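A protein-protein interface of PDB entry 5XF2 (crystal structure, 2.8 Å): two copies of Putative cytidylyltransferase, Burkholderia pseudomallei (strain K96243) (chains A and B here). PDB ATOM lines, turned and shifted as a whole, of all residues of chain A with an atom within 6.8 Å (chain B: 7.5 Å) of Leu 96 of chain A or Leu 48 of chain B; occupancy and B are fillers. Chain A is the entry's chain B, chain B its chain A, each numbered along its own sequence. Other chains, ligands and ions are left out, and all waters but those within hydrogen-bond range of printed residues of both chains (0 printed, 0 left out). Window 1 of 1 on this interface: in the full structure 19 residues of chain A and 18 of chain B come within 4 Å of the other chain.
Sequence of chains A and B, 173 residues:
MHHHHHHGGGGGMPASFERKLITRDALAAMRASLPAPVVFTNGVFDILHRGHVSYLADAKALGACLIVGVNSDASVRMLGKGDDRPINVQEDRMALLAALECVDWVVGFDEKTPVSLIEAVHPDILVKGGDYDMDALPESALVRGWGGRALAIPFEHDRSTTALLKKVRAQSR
The guanidinium group (NH2) of Arg 50 of chain B lies within salt-bridge range of the side-chain carboxylate (OE1) of Glu 91 of chain A, 3.5 Å away. The guanidinium group (NH1) of Arg 50 of chain B is in salt-bridge range of the side-chain carboxylate (OD1) of Asp 92 of chain A, at 2.9 Å.
A ring nitrogen (ND1) of His 52 of chain B lies close to the backbone carbonyl oxygen (O) of Ile 47 of chain B (3.5 Å). A ring nitrogen (ND1) of His 49 of chain B sits at hydrogen-bond distance from the backbone NH (N) of Gly 51 of chain B (3.0 Å). A ring nitrogen (ND1) of His 52 of chain B sits at hydrogen-bond distance from the backbone NH (N) of His 49 of chain B (3.2 Å). O of Arg 50 of chain B sits at hydrogen-bond distance from OG of Ser 54 of chain B (3.0 Å).
Val 53 of chain B touches Phe 17 of chain A (O to CE2, 3.9 Å). CG2 of Ile 47 of chain B touches CG2 of Ile 47 of chain A (3.8 Å). Arg 50 of chain B touches Ala 95 of chain A. Leu 48 of chain B touches Leu 96 of chain A. Leu 96 of chain A touches His 49 of chain B (CD2 to C, 3.7 Å). Leu 96 of chain A touches Arg 50 of chain B (CD2 to N, 3.6 Å). O of Ala 99 of chain A touches CA of Leu 100 of chain B, 3.5 Å away. Ala 99 of chain B touches Leu 100 of chain A.
Of the printed residues of chain B, Ala 95 of chain A touches Arg 50. Of chain B, only Leu 48 (3.97 Å), His 49 (3.7 Å) and Arg 50 (3.6 Å) come within 4 Å of Leu 96 of chain A. Leu 97 of chain A touches none of the printed residues of chain B. Of the printed residues of chain B, Leu 100 of chain A touches Ala 99 (3.5 Å). Of the printed residues of chain A, Ile 47 of chain B touches Ile 47 (3.8 Å). Leu 48 of chain B touches just one residue of chain A: Leu 96 (3.97 Å). Printed residues of chain A within 4 Å of Arg 50 of chain B: Glu 91 (3.5 Å), Asp 92 (2.9 Å), Ala 95 (3.8 Å) and Leu 96 (3.6 Å). Of the printed residues of chain A, Ala 99 of chain B touches Leu 100. Of the printed residues of chain A, Leu 100 of chain B touches Ala 99 (3.5 Å).
Of the 19 printed residues of chain B, 7 touch a printed residue of chain A. Among the printed residues, Asp or Glu carboxylates within 4 Å of a Lys or Arg side-chain nitrogen of the other chain: Glu 91 of chain A with Arg 50 of chain B and Asp 92 of chain A with Arg 50 of chain B.
Ile 47 of chain A touches its own counterpart, Ile 47 of chain B. Leu 96 of chain A touches Leu 48 of chain B, but with the chains exchanged Leu 48 of chain A does not touch Leu 96 of chain B (4.04 Å). Ala 99 of chain A touches Leu 100 of chain B, and with the chains exchanged Leu 100 of chain A touches Ala 99 of chain B.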
ATOM      1  N   PHE A  17     -28.971  -2.835   6.438  1.00  0.00           N
ATOM      2  CA  PHE A  17     -28.357  -1.721   5.715  1.00  0.00           C
ATOM      3  C   PHE A  17     -26.947  -1.989   5.187  1.00  0.00           C
ATOM      4  O   PHE A  17     -26.489  -1.328   4.256  1.00  0.00           O
ATOM      5  CB  PHE A  17     -28.351  -0.461   6.586  1.00  0.00           C
ATOM      6  CG  PHE A  17     -27.495  -0.578   7.815  1.00  0.00           C
ATOM      7  CD1 PHE A  17     -26.112  -0.581   7.713  1.00  0.00           C
ATOM      8  CD2 PHE A  17     -28.068  -0.683   9.069  1.00  0.00           C
ATOM      9  CE1 PHE A  17     -25.319  -0.687   8.840  1.00  0.00           C
ATOM     10  CE2 PHE A  17     -27.282  -0.792  10.200  1.00  0.00           C
ATOM     11  CZ  PHE A  17     -25.906  -0.793  10.087  1.00  0.00           C
ATOM     12  N   LEU A  21     -22.789  -1.891   1.580  1.00  0.00           N
ATOM     13  CA  LEU A  21     -21.336  -1.770   1.586  1.00  0.00           C
ATOM     14  C   LEU A  21     -20.771  -2.803   0.619  1.00  0.00           C
ATOM     15  O   LEU A  21     -20.910  -4.005   0.842  1.00  0.00           O
ATOM     16  CB  LEU A  21     -20.781  -1.999   2.992  1.00  0.00           C
ATOM     17  CG  LEU A  21     -21.345  -1.103   4.097  1.00  0.00           C
ATOM     18  CD1 LEU A  21     -21.026  -1.676   5.469  1.00  0.00           C
ATOM     19  CD2 LEU A  21     -20.809   0.313   3.966  1.00  0.00           C
ATOM     20  N   PHE A  45     -17.031  12.304   4.766  1.00  0.00           N
ATOM     21  CA  PHE A  45     -18.208  12.112   5.604  1.00  0.00           C
ATOM     22  C   PHE A  45     -17.831  11.643   7.001  1.00  0.00           C
ATOM     23  O   PHE A  45     -18.330  10.625   7.482  1.00  0.00           O
ATOM     24  CB  PHE A  45     -19.170  11.112   4.956  1.00  0.00           C
ATOM     25  CG  PHE A  45     -19.702  11.560   3.626  1.00  0.00           C
ATOM     26  CD1 PHE A  45     -20.721  12.495   3.549  1.00  0.00           C
ATOM     27  CD2 PHE A  45     -19.183  11.045   2.449  1.00  0.00           C
ATOM     28  CE1 PHE A  45     -21.214  12.908   2.328  1.00  0.00           C
ATOM     29  CE2 PHE A  45     -19.670  11.454   1.221  1.00  0.00           C
ATOM     30  CZ  PHE A  45     -20.688  12.386   1.160  1.00  0.00           C
ATOM     31  N   ASP A  46     -16.948  12.395   7.649  1.00  0.00           N
ATOM     32  CA  ASP A  46     -16.498  12.066   8.996  1.00  0.00           C
ATOM     33  C   ASP A  46     -17.662  12.044   9.979  1.00  0.00           C
ATOM     34  O   ASP A  46     -18.021  10.991  10.505  1.00  0.00           O
ATOM     35  CB  ASP A  46     -15.434  13.062   9.463  1.00  0.00           C
ATOM     36  CG  ASP A  46     -14.468  12.458  10.464  1.00  0.00           C
ATOM     37  OD1 ASP A  46     -14.727  11.330  10.936  1.00  0.00           O
ATOM     38  OD2 ASP A  46     -13.450  13.109  10.780  1.00  0.00           O
ATOM     39  N   ILE A  47     -18.249  13.211  10.225  1.00  0.00           N
ATOM     40  CA  ILE A  47     -19.371  13.314  11.146  1.00  0.00           C
ATOM     41  C   ILE A  47     -20.550  13.800  10.327  1.00  0.00           C
ATOM     42  O   ILE A  47     -20.490  14.883   9.736  1.00  0.00           O
ATOM     43  CB  ILE A  47     -19.084  14.309  12.326  1.00  0.00           C
ATOM     44  CG1 ILE A  47     -17.952  13.811  13.225  1.00  0.00           C
ATOM     45  CG2 ILE A  47     -20.363  14.645  13.115  1.00  0.00           C
ATOM     46  CD1 ILE A  47     -16.617  14.477  12.934  1.00  0.00           C
ATOM     47  N   LEU A  48     -21.607  13.004  10.258  1.00  0.00           N
ATOM     48  CA  LEU A  48     -22.777  13.423   9.500  1.00  0.00           C
ATOM     49  C   LEU A  48     -23.478  14.612  10.136  1.00  0.00           C
ATOM     50  O   LEU A  48     -23.605  14.694  11.355  1.00  0.00           O
ATOM     51  CB  LEU A  48     -23.782  12.284   9.357  1.00  0.00           C
ATOM     52  CG  LEU A  48     -23.437  11.249   8.297  1.00  0.00           C
ATOM     53  CD1 LEU A  48     -24.581  10.267   8.190  1.00  0.00           C
ATOM     54  CD2 LEU A  48     -23.152  11.920   6.962  1.00  0.00           C
ATOM     55  N   ASN A  88     -13.529   9.080  12.689  1.00  0.00           N
ATOM     56  CA  ASN A  88     -14.120   7.755  12.597  1.00  0.00           C
ATOM     57  C   ASN A  88     -13.404   6.963  11.518  1.00  0.00           C
ATOM     58  O   ASN A  88     -13.035   7.508  10.480  1.00  0.00           O
ATOM     59  CB  ASN A  88     -15.614   7.845  12.306  1.00  0.00           C
ATOM     60  CG  ASN A  88     -16.401   8.413  13.459  1.00  0.00           C
ATOM     61  OD1 ASN A  88     -17.050   9.455  13.334  1.00  0.00           O
ATOM     62  ND2 ASN A  88     -16.361   7.730  14.591  1.00  0.00           N
ATOM     63  N   GLU A  91     -14.757   2.169   7.932  1.00  0.00           N
ATOM     64  CA  GLU A  91     -15.930   1.302   7.947  1.00  0.00           C
ATOM     65  C   GLU A  91     -17.084   1.926   8.726  1.00  0.00           C
ATOM     66  O   GLU A  91     -18.237   1.671   8.405  1.00  0.00           O
ATOM     67  CB  GLU A  91     -15.609  -0.100   8.466  1.00  0.00           C
ATOM     68  CG  GLU A  91     -16.066  -1.132   7.428  1.00  0.00           C
ATOM     69  CD  GLU A  91     -16.155  -2.554   7.942  1.00  0.00           C
ATOM     70  OE1 GLU A  91     -16.977  -2.820   8.851  1.00  0.00           O
ATOM     71  OE2 GLU A  91     -15.418  -3.416   7.404  1.00  0.00           O
ATOM     72  N   ASP A  92     -16.787   2.756   9.723  1.00  0.00           N
ATOM     73  CA  ASP A  92     -17.851   3.413  10.481  1.00  0.00           C
ATOM     74  C   ASP A  92     -18.483   4.525   9.648  1.00  0.00           C
ATOM     75  O   ASP A  92     -19.706   4.740   9.694  1.00  0.00           O
ATOM     76  CB  ASP A  92     -17.330   3.993  11.806  1.00  0.00           C
ATOM     77  CG  ASP A  92     -17.115   2.924  12.884  1.00  0.00           C
ATOM     78  OD1 ASP A  92     -17.079   1.721  12.534  1.00  0.00           O
ATOM     79  OD2 ASP A  92     -17.041   3.285  14.089  1.00  0.00           O
ATOM     80  N   ARG A  93     -17.650   5.244   8.901  1.00  0.00           N
ATOM     81  CA  ARG A  93     -18.127   6.313   8.038  1.00  0.00           C
ATOM     82  C   ARG A  93     -18.986   5.721   6.917  1.00  0.00           C
ATOM     83  O   ARG A  93     -20.015   6.294   6.522  1.00  0.00           O
ATOM     84  CB  ARG A  93     -16.946   7.116   7.476  1.00  0.00           C
ATOM     85  CG  ARG A  93     -16.238   7.966   8.534  1.00  0.00           C
ATOM     86  CD  ARG A  93     -15.096   8.816   7.933  1.00  0.00           C
ATOM     87  NE  ARG A  93     -13.893   8.042   7.609  1.00  0.00           N
ATOM     88  CZ  ARG A  93     -13.399   7.897   6.381  1.00  0.00           C
ATOM     89  NH1 ARG A  93     -14.005   8.473   5.349  1.00  0.00           N
ATOM     90  NH2 ARG A  93     -12.304   7.182   6.175  1.00  0.00           N
ATOM     91  N   MET A  94     -18.585   4.551   6.431  1.00  0.00           N
ATOM     92  CA  MET A  94     -19.334   3.895   5.368  1.00  0.00           C
ATOM     93  C   MET A  94     -20.657   3.322   5.906  1.00  0.00           C
ATOM     94  O   MET A  94     -21.708   3.431   5.259  1.00  0.00           O
ATOM     95  CB  MET A  94     -18.496   2.769   4.763  1.00  0.00           C
ATOM     96  CG  MET A  94     -17.281   3.261   3.992  1.00  0.00           C
ATOM     97  SD  MET A  94     -16.164   1.865   3.298  1.00  0.00           S
ATOM     98  CE  MET A  94     -17.347   1.240   1.880  1.00  0.00           C
ATOM     99  N   ALA A  95     -20.612   2.738   7.099  1.00  0.00           N
ATOM    100  CA  ALA A  95     -21.823   2.223   7.746  1.00  0.00           C
ATOM    101  C   ALA A  95     -22.859   3.325   8.006  1.00  0.00           C
ATOM    102  O   ALA A  95     -24.051   3.113   7.814  1.00  0.00           O
ATOM    103  CB  ALA A  95     -21.469   1.523   9.057  1.00  0.00           C
ATOM    104  N   LEU A  96     -22.414   4.494   8.451  1.00  0.00           N
ATOM    105  CA  LEU A  96     -23.333   5.597   8.705  1.00  0.00           C
ATOM    106  C   LEU A  96     -24.091   5.959   7.435  1.00  0.00           C
ATOM    107  O   LEU A  96     -25.321   6.056   7.427  1.00  0.00           O
ATOM    108  CB  LEU A  96     -22.573   6.809   9.259  1.00  0.00           C
ATOM    109  CG  LEU A  96     -22.702   6.948  10.778  1.00  0.00           C
ATOM    110  CD1 LEU A  96     -24.047   7.545  11.150  1.00  0.00           C
ATOM    111  CD2 LEU A  96     -22.539   5.588  11.464  1.00  0.00           C
ATOM    112  N   LEU A  97     -23.344   6.118   6.347  1.00  0.00           N
ATOM    113  CA  LEU A  97     -23.931   6.415   5.049  1.00  0.00           C
ATOM    114  C   LEU A  97     -24.889   5.333   4.578  1.00  0.00           C
ATOM    115  O   LEU A  97     -25.963   5.634   4.052  1.00  0.00           O
ATOM    116  CB  LEU A  97     -22.820   6.609   4.004  1.00  0.00           C
ATOM    117  CG  LEU A  97     -22.076   7.917   4.201  1.00  0.00           C
ATOM    118  CD1 LEU A  97     -20.746   7.912   3.501  1.00  0.00           C
ATOM    119  CD2 LEU A  97     -22.941   9.049   3.709  1.00  0.00           C
ATOM    120  N   ALA A  98     -24.509   4.071   4.769  1.00  0.00           N
ATOM    121  CA  ALA A  98     -25.324   2.970   4.259  1.00  0.00           C
ATOM    122  C   ALA A  98     -26.681   2.927   4.967  1.00  0.00           C
ATOM    123  O   ALA A  98     -27.658   2.399   4.430  1.00  0.00           O
ATOM    124  CB  ALA A  98     -24.593   1.647   4.419  1.00  0.00           C
ATOM    125  N   ALA A  99     -26.729   3.469   6.179  1.00  0.00           N
ATOM    126  CA  ALA A  99     -27.962   3.518   6.963  1.00  0.00           C
ATOM    127  C   ALA A  99     -28.932   4.558   6.423  1.00  0.00           C
ATOM    128  O   ALA A  99     -30.090   4.589   6.820  1.00  0.00           O
ATOM    129  CB  ALA A  99     -27.649   3.811   8.423  1.00  0.00           C
ATOM    130  N   LEU A 100     -28.473   5.420   5.524  1.00  0.00           N
ATOM    131  CA  LEU A 100     -29.354   6.465   5.027  1.00  0.00           C
ATOM    132  C   LEU A 100     -30.314   5.910   3.996  1.00  0.00           C
ATOM    133  O   LEU A 100     -29.927   5.133   3.124  1.00  0.00           O
ATOM    134  CB  LEU A 100     -28.555   7.631   4.438  1.00  0.00           C
ATOM    135  CG  LEU A 100     -27.751   8.400   5.493  1.00  0.00           C
ATOM    136  CD1 LEU A 100     -26.939   9.499   4.841  1.00  0.00           C
ATOM    137  CD2 LEU A 100     -28.677   8.975   6.558  1.00  0.00           C
ATOM    138  N   VAL A 103     -29.371   6.441   0.154  1.00  0.00           N
ATOM    139  CA  VAL A 103     -28.114   5.901  -0.355  1.00  0.00           C
ATOM    140  C   VAL A 103     -28.303   4.476  -0.850  1.00  0.00           C
ATOM    141  O   VAL A 103     -28.933   3.673  -0.156  1.00  0.00           O
ATOM    142  CB  VAL A 103     -27.022   5.918   0.740  1.00  0.00           C
ATOM    143  CG1 VAL A 103     -25.783   5.192   0.280  1.00  0.00           C
ATOM    144  CG2 VAL A 103     -26.665   7.340   1.125  1.00  0.00           C
ATOM    145  N   VAL A 106     -22.370   2.023  -1.042  1.00  0.00           N
ATOM    146  CA  VAL A 106     -21.237   2.745  -0.462  1.00  0.00           C
ATOM    147  C   VAL A 106     -19.951   1.969  -0.764  1.00  0.00           C
ATOM    148  O   VAL A 106     -19.865   0.772  -0.449  1.00  0.00           O
ATOM    149  CB  VAL A 106     -21.401   2.938   1.053  1.00  0.00           C
ATOM    150  CG1 VAL A 106     -20.308   3.832   1.597  1.00  0.00           C
ATOM    151  CG2 VAL A 106     -22.781   3.525   1.380  1.00  0.00           C
ATOM    152  N   PHE B  45     -29.544  11.742  20.637  1.00  0.00           N
ATOM    153  CA  PHE B  45     -28.984  11.521  19.322  1.00  0.00           C
ATOM    154  C   PHE B  45     -28.302  12.792  18.805  1.00  0.00           C
ATOM    155  O   PHE B  45     -28.559  13.196  17.664  1.00  0.00           O
ATOM    156  CB  PHE B  45     -30.075  11.058  18.351  1.00  0.00           C
ATOM    157  CG  PHE B  45     -30.719   9.751  18.738  1.00  0.00           C
ATOM    158  CD1 PHE B  45     -30.069   8.553  18.525  1.00  0.00           C
ATOM    159  CD2 PHE B  45     -31.982   9.722  19.288  1.00  0.00           C
ATOM    160  CE1 PHE B  45     -30.657   7.345  18.871  1.00  0.00           C
ATOM    161  CE2 PHE B  45     -32.581   8.514  19.627  1.00  0.00           C
ATOM    162  CZ  PHE B  45     -31.915   7.331  19.423  1.00  0.00           C
ATOM    163  N   ASP B  46     -27.438  13.396  19.639  1.00  0.00           N
ATOM    164  CA  ASP B  46     -26.724  14.646  19.294  1.00  0.00           C
ATOM    165  C   ASP B  46     -25.840  14.452  18.074  1.00  0.00           C
ATOM    166  O   ASP B  46     -25.985  15.150  17.078  1.00  0.00           O
ATOM    167  CB  ASP B  46     -25.860  15.153  20.461  1.00  0.00           C
ATOM    168  CG  ASP B  46     -25.652  16.688  20.428  1.00  0.00           C
ATOM    169  OD1 ASP B  46     -26.145  17.347  19.482  1.00  0.00           O
ATOM    170  OD2 ASP B  46     -24.933  17.233  21.306  1.00  0.00           O
ATOM    171  N   ILE B  47     -24.901  13.517  18.177  1.00  0.00           N
ATOM    172  CA  ILE B  47     -24.066  13.087  17.054  1.00  0.00           C
ATOM    173  C   ILE B  47     -24.283  11.609  16.807  1.00  0.00           C
ATOM    174  O   ILE B  47     -24.029  10.799  17.697  1.00  0.00           O
ATOM    175  CB  ILE B  47     -22.566  13.336  17.295  1.00  0.00           C
ATOM    176  CG1 ILE B  47     -22.295  14.831  17.364  1.00  0.00           C
ATOM    177  CG2 ILE B  47     -21.736  12.798  16.146  1.00  0.00           C
ATOM    178  CD1 ILE B  47     -20.918  15.144  17.855  1.00  0.00           C
ATOM    179  N   LEU B  48     -24.782  11.258  15.621  1.00  0.00           N
ATOM    180  CA  LEU B  48     -25.012   9.856  15.289  1.00  0.00           C
ATOM    181  C   LEU B  48     -23.696   9.139  15.156  1.00  0.00           C
ATOM    182  O   LEU B  48     -22.785   9.624  14.484  1.00  0.00           O
ATOM    183  CB  LEU B  48     -25.805   9.696  13.993  1.00  0.00           C
ATOM    184  CG  LEU B  48     -27.321   9.814  14.002  1.00  0.00           C
ATOM    185  CD1 LEU B  48     -27.838   9.514  12.619  1.00  0.00           C
ATOM    186  CD2 LEU B  48     -27.867   8.794  14.951  1.00  0.00           C
ATOM    187  N   HIS B  49     -23.617   7.959  15.754  1.00  0.00           N
ATOM    188  CA  HIS B  49     -22.476   7.097  15.543  1.00  0.00           C
ATOM    189  C   HIS B  49     -22.992   5.714  15.178  1.00  0.00           C
ATOM    190  O   HIS B  49     -24.204   5.485  15.142  1.00  0.00           O
ATOM    191  CB  HIS B  49     -21.577   7.040  16.780  1.00  0.00           C
ATOM    192  CG  HIS B  49     -22.300   6.673  18.033  1.00  0.00           C
ATOM    193  ND1 HIS B  49     -22.771   5.396  18.277  1.00  0.00           N
ATOM    194  CD2 HIS B  49     -22.566   7.388  19.155  1.00  0.00           C
ATOM    195  CE1 HIS B  49     -23.346   5.358  19.466  1.00  0.00           C
ATOM    196  NE2 HIS B  49     -23.236   6.555  20.019  1.00  0.00           N
ATOM    197  N   ARG B  50     -22.071   4.799  14.904  1.00  0.00           N
ATOM    198  CA  ARG B  50     -22.429   3.488  14.396  1.00  0.00           C
ATOM    199  C   ARG B  50     -23.272   2.655  15.368  1.00  0.00           C
ATOM    200  O   ARG B  50     -24.097   1.848  14.941  1.00  0.00           O
ATOM    201  CB  ARG B  50     -21.161   2.730  14.014  1.00  0.00           C
ATOM    202  CG  ARG B  50     -21.438   1.438  13.304  1.00  0.00           C
ATOM    203  CD  ARG B  50     -20.166   0.715  12.990  1.00  0.00           C
ATOM    204  NE  ARG B  50     -20.446  -0.426  12.137  1.00  0.00           N
ATOM    205  CZ  ARG B  50     -19.529  -1.060  11.420  1.00  0.00           C
ATOM    206  NH1 ARG B  50     -18.260  -0.665  11.465  1.00  0.00           N
ATOM    207  NH2 ARG B  50     -19.885  -2.096  10.667  1.00  0.00           N
ATOM    208  N   GLY B  51     -23.073   2.851  16.666  1.00  0.00           N
ATOM    209  CA  GLY B  51     -23.863   2.146  17.667  1.00  0.00           C
ATOM    210  C   GLY B  51     -25.326   2.549  17.606  1.00  0.00           C
ATOM    211  O   GLY B  51     -26.217   1.711  17.701  1.00  0.00           O
ATOM    212  N   HIS B  52     -25.561   3.841  17.419  1.00  0.00           N
ATOM    213  CA  HIS B  52     -26.898   4.380  17.246  1.00  0.00           C
ATOM    214  C   HIS B  52     -27.639   3.708  16.097  1.00  0.00           C
ATOM    215  O   HIS B  52     -28.763   3.252  16.265  1.00  0.00           O
ATOM    216  CB  HIS B  52     -26.826   5.874  16.972  1.00  0.00           C
ATOM    217  CG  HIS B  52     -26.540   6.704  18.180  1.00  0.00           C
ATOM    218  ND1 HIS B  52     -25.626   7.733  18.171  1.00  0.00           N
ATOM    219  CD2 HIS B  52     -27.068   6.682  19.426  1.00  0.00           C
ATOM    220  CE1 HIS B  52     -25.606   8.311  19.357  1.00  0.00           C
ATOM    221  NE2 HIS B  52     -26.472   7.694  20.137  1.00  0.00           N
ATOM    222  N   VAL B  53     -27.024   3.651  14.920  1.00  0.00           N
ATOM    223  CA  VAL B  53     -27.738   3.128  13.759  1.00  0.00           C
ATOM    224  C   VAL B  53     -27.844   1.613  13.781  1.00  0.00           C
ATOM    225  O   VAL B  53     -28.834   1.070  13.299  1.00  0.00           O
ATOM    226  CB  VAL B  53     -27.111   3.611  12.419  1.00  0.00           C
ATOM    227  CG1 VAL B  53     -27.198   5.157  12.332  1.00  0.00           C
ATOM    228  CG2 VAL B  53     -25.686   3.120  12.252  1.00  0.00           C
ATOM    229  N   SER B  54     -26.846   0.938  14.343  1.00  0.00           N
ATOM    230  CA  SER B  54     -26.873  -0.515  14.432  1.00  0.00           C
ATOM    231  C   SER B  54     -28.061  -0.903  15.303  1.00  0.00           C
ATOM    232  O   SER B  54     -28.819  -1.817  14.977  1.00  0.00           O
ATOM    233  CB  SER B  54     -25.573  -1.045  15.037  1.00  0.00           C
ATOM    234  OG  SER B  54     -24.514  -0.986  14.098  1.00  0.00           O
ATOM    235  N   LEU B  56     -30.625   1.153  16.013  1.00  0.00           N
ATOM    236  CA  LEU B  56     -31.874   1.647  15.433  1.00  0.00           C
ATOM    237  C   LEU B  56     -32.443   0.639  14.428  1.00  0.00           C
ATOM    238  O   LEU B  56     -33.658   0.501  14.283  1.00  0.00           O
ATOM    239  CB  LEU B  56     -31.653   3.000  14.756  1.00  0.00           C
ATOM    240  CG  LEU B  56     -31.679   4.227  15.670  1.00  0.00           C
ATOM    241  CD1 LEU B  56     -31.676   5.508  14.849  1.00  0.00           C
ATOM    242  CD2 LEU B  56     -32.884   4.182  16.597  1.00  0.00           C
ATOM    243  N   ASN B  88     -26.461  20.393  18.513  1.00  0.00           N
ATOM    244  CA  ASN B  88     -27.376  20.405  17.422  1.00  0.00           C
ATOM    245  C   ASN B  88     -28.694  20.635  18.041  1.00  0.00           C
ATOM    246  O   ASN B  88     -29.016  20.129  19.115  1.00  0.00           O
ATOM    247  CB  ASN B  88     -27.361  19.065  16.690  1.00  0.00           C
ATOM    248  CG  ASN B  88     -26.321  19.013  15.588  1.00  0.00           C
ATOM    249  OD1 ASN B  88     -26.173  19.961  14.814  1.00  0.00           O
ATOM    250  ND2 ASN B  88     -25.594  17.906  15.511  1.00  0.00           N
ATOM    251  N   ARG B  93     -31.340  17.300  15.041  1.00  0.00           N
ATOM    252  CA  ARG B  93     -31.167  15.953  15.564  1.00  0.00           C
ATOM    253  C   ARG B  93     -32.271  15.054  15.044  1.00  0.00           C
ATOM    254  O   ARG B  93     -32.007  13.923  14.659  1.00  0.00           O
ATOM    255  CB  ARG B  93     -31.148  15.953  17.085  1.00  0.00           C
ATOM    256  CG  ARG B  93     -29.869  16.522  17.653  1.00  0.00           C
ATOM    257  CD  ARG B  93     -29.856  16.478  19.168  1.00  0.00           C
ATOM    258  NE  ARG B  93     -30.683  17.523  19.761  1.00  0.00           N
ATOM    259  CZ  ARG B  93     -31.685  17.290  20.605  1.00  0.00           C
ATOM    260  NH1 ARG B  93     -31.991  16.043  20.949  1.00  0.00           N
ATOM    261  NH2 ARG B  93     -32.390  18.302  21.099  1.00  0.00           N
ATOM    262  N   ALA B  95     -34.031  15.576  12.201  1.00  0.00           N
ATOM    263  CA  ALA B  95     -33.870  15.414  10.757  1.00  0.00           C
ATOM    264  C   ALA B  95     -32.889  14.287  10.393  1.00  0.00           C
ATOM    265  O   ALA B  95     -33.159  13.494   9.474  1.00  0.00           O
ATOM    266  CB  ALA B  95     -33.438  16.736  10.122  1.00  0.00           C
ATOM    267  N   LEU B  96     -31.765  14.199  11.109  1.00  0.00           N
ATOM    268  CA  LEU B  96     -30.792  13.137  10.872  1.00  0.00           C
ATOM    269  C   LEU B  96     -31.438  11.784  11.033  1.00  0.00           C
ATOM    270  O   LEU B  96     -31.288  10.917  10.175  1.00  0.00           O
ATOM    271  CB  LEU B  96     -29.616  13.243  11.829  1.00  0.00           C
ATOM    272  CG  LEU B  96     -28.336  13.830  11.286  1.00  0.00           C
ATOM    273  CD1 LEU B  96     -27.634  12.778  10.484  1.00  0.00           C
ATOM    274  CD2 LEU B  96     -28.697  15.013  10.423  1.00  0.00           C
ATOM    275  N   LEU B  97     -32.173  11.604  12.129  1.00  0.00           N
ATOM    276  CA  LEU B  97     -32.872  10.346  12.377  1.00  0.00           C
ATOM    277  C   LEU B  97     -33.832  10.018  11.240  1.00  0.00           C
ATOM    278  O   LEU B  97     -33.923   8.865  10.792  1.00  0.00           O
ATOM    279  CB  LEU B  97     -33.613  10.428  13.712  1.00  0.00           C
ATOM    280  CG  LEU B  97     -32.619  10.390  14.871  1.00  0.00           C
ATOM    281  CD1 LEU B  97     -33.188  10.938  16.160  1.00  0.00           C
ATOM    282  CD2 LEU B  97     -32.177   8.949  15.069  1.00  0.00           C
ATOM    283  N   ALA B  98     -34.545  11.026  10.751  1.00  0.00           N
ATOM    284  CA  ALA B  98     -35.534  10.782   9.713  1.00  0.00           C
ATOM    285  C   ALA B  98     -34.881  10.310   8.414  1.00  0.00           C
ATOM    286  O   ALA B  98     -35.504   9.597   7.626  1.00  0.00           O
ATOM    287  CB  ALA B  98     -36.372  12.030   9.469  1.00  0.00           C
ATOM    288  N   ALA B  99     -33.620  10.671   8.211  1.00  0.00           N
ATOM    289  CA  ALA B  99     -32.899  10.301   6.993  1.00  0.00           C
ATOM    290  C   ALA B  99     -32.575   8.820   6.983  1.00  0.00           C
ATOM    291  O   ALA B  99     -32.172   8.273   5.947  1.00  0.00           O
ATOM    292  CB  ALA B  99     -31.628  11.118   6.848  1.00  0.00           C
ATOM    293  N   LEU B 100     -32.760   8.175   8.129  1.00  0.00           N
ATOM    294  CA  LEU B 100     -32.419   6.770   8.285  1.00  0.00           C
ATOM    295  C   LEU B 100     -33.469   5.843   7.678  1.00  0.00           C
ATOM    296  O   LEU B 100     -34.680   6.035   7.856  1.00  0.00           O
ATOM    297  CB  LEU B 100     -32.249   6.450   9.770  1.00  0.00           C
ATOM    298  CG  LEU B 100     -31.074   7.189  10.400  1.00  0.00           C
ATOM    299  CD1 LEU B 100     -31.012   6.958  11.899  1.00  0.00           C
ATOM    300  CD2 LEU B 100     -29.775   6.746   9.705  1.00  0.00           C
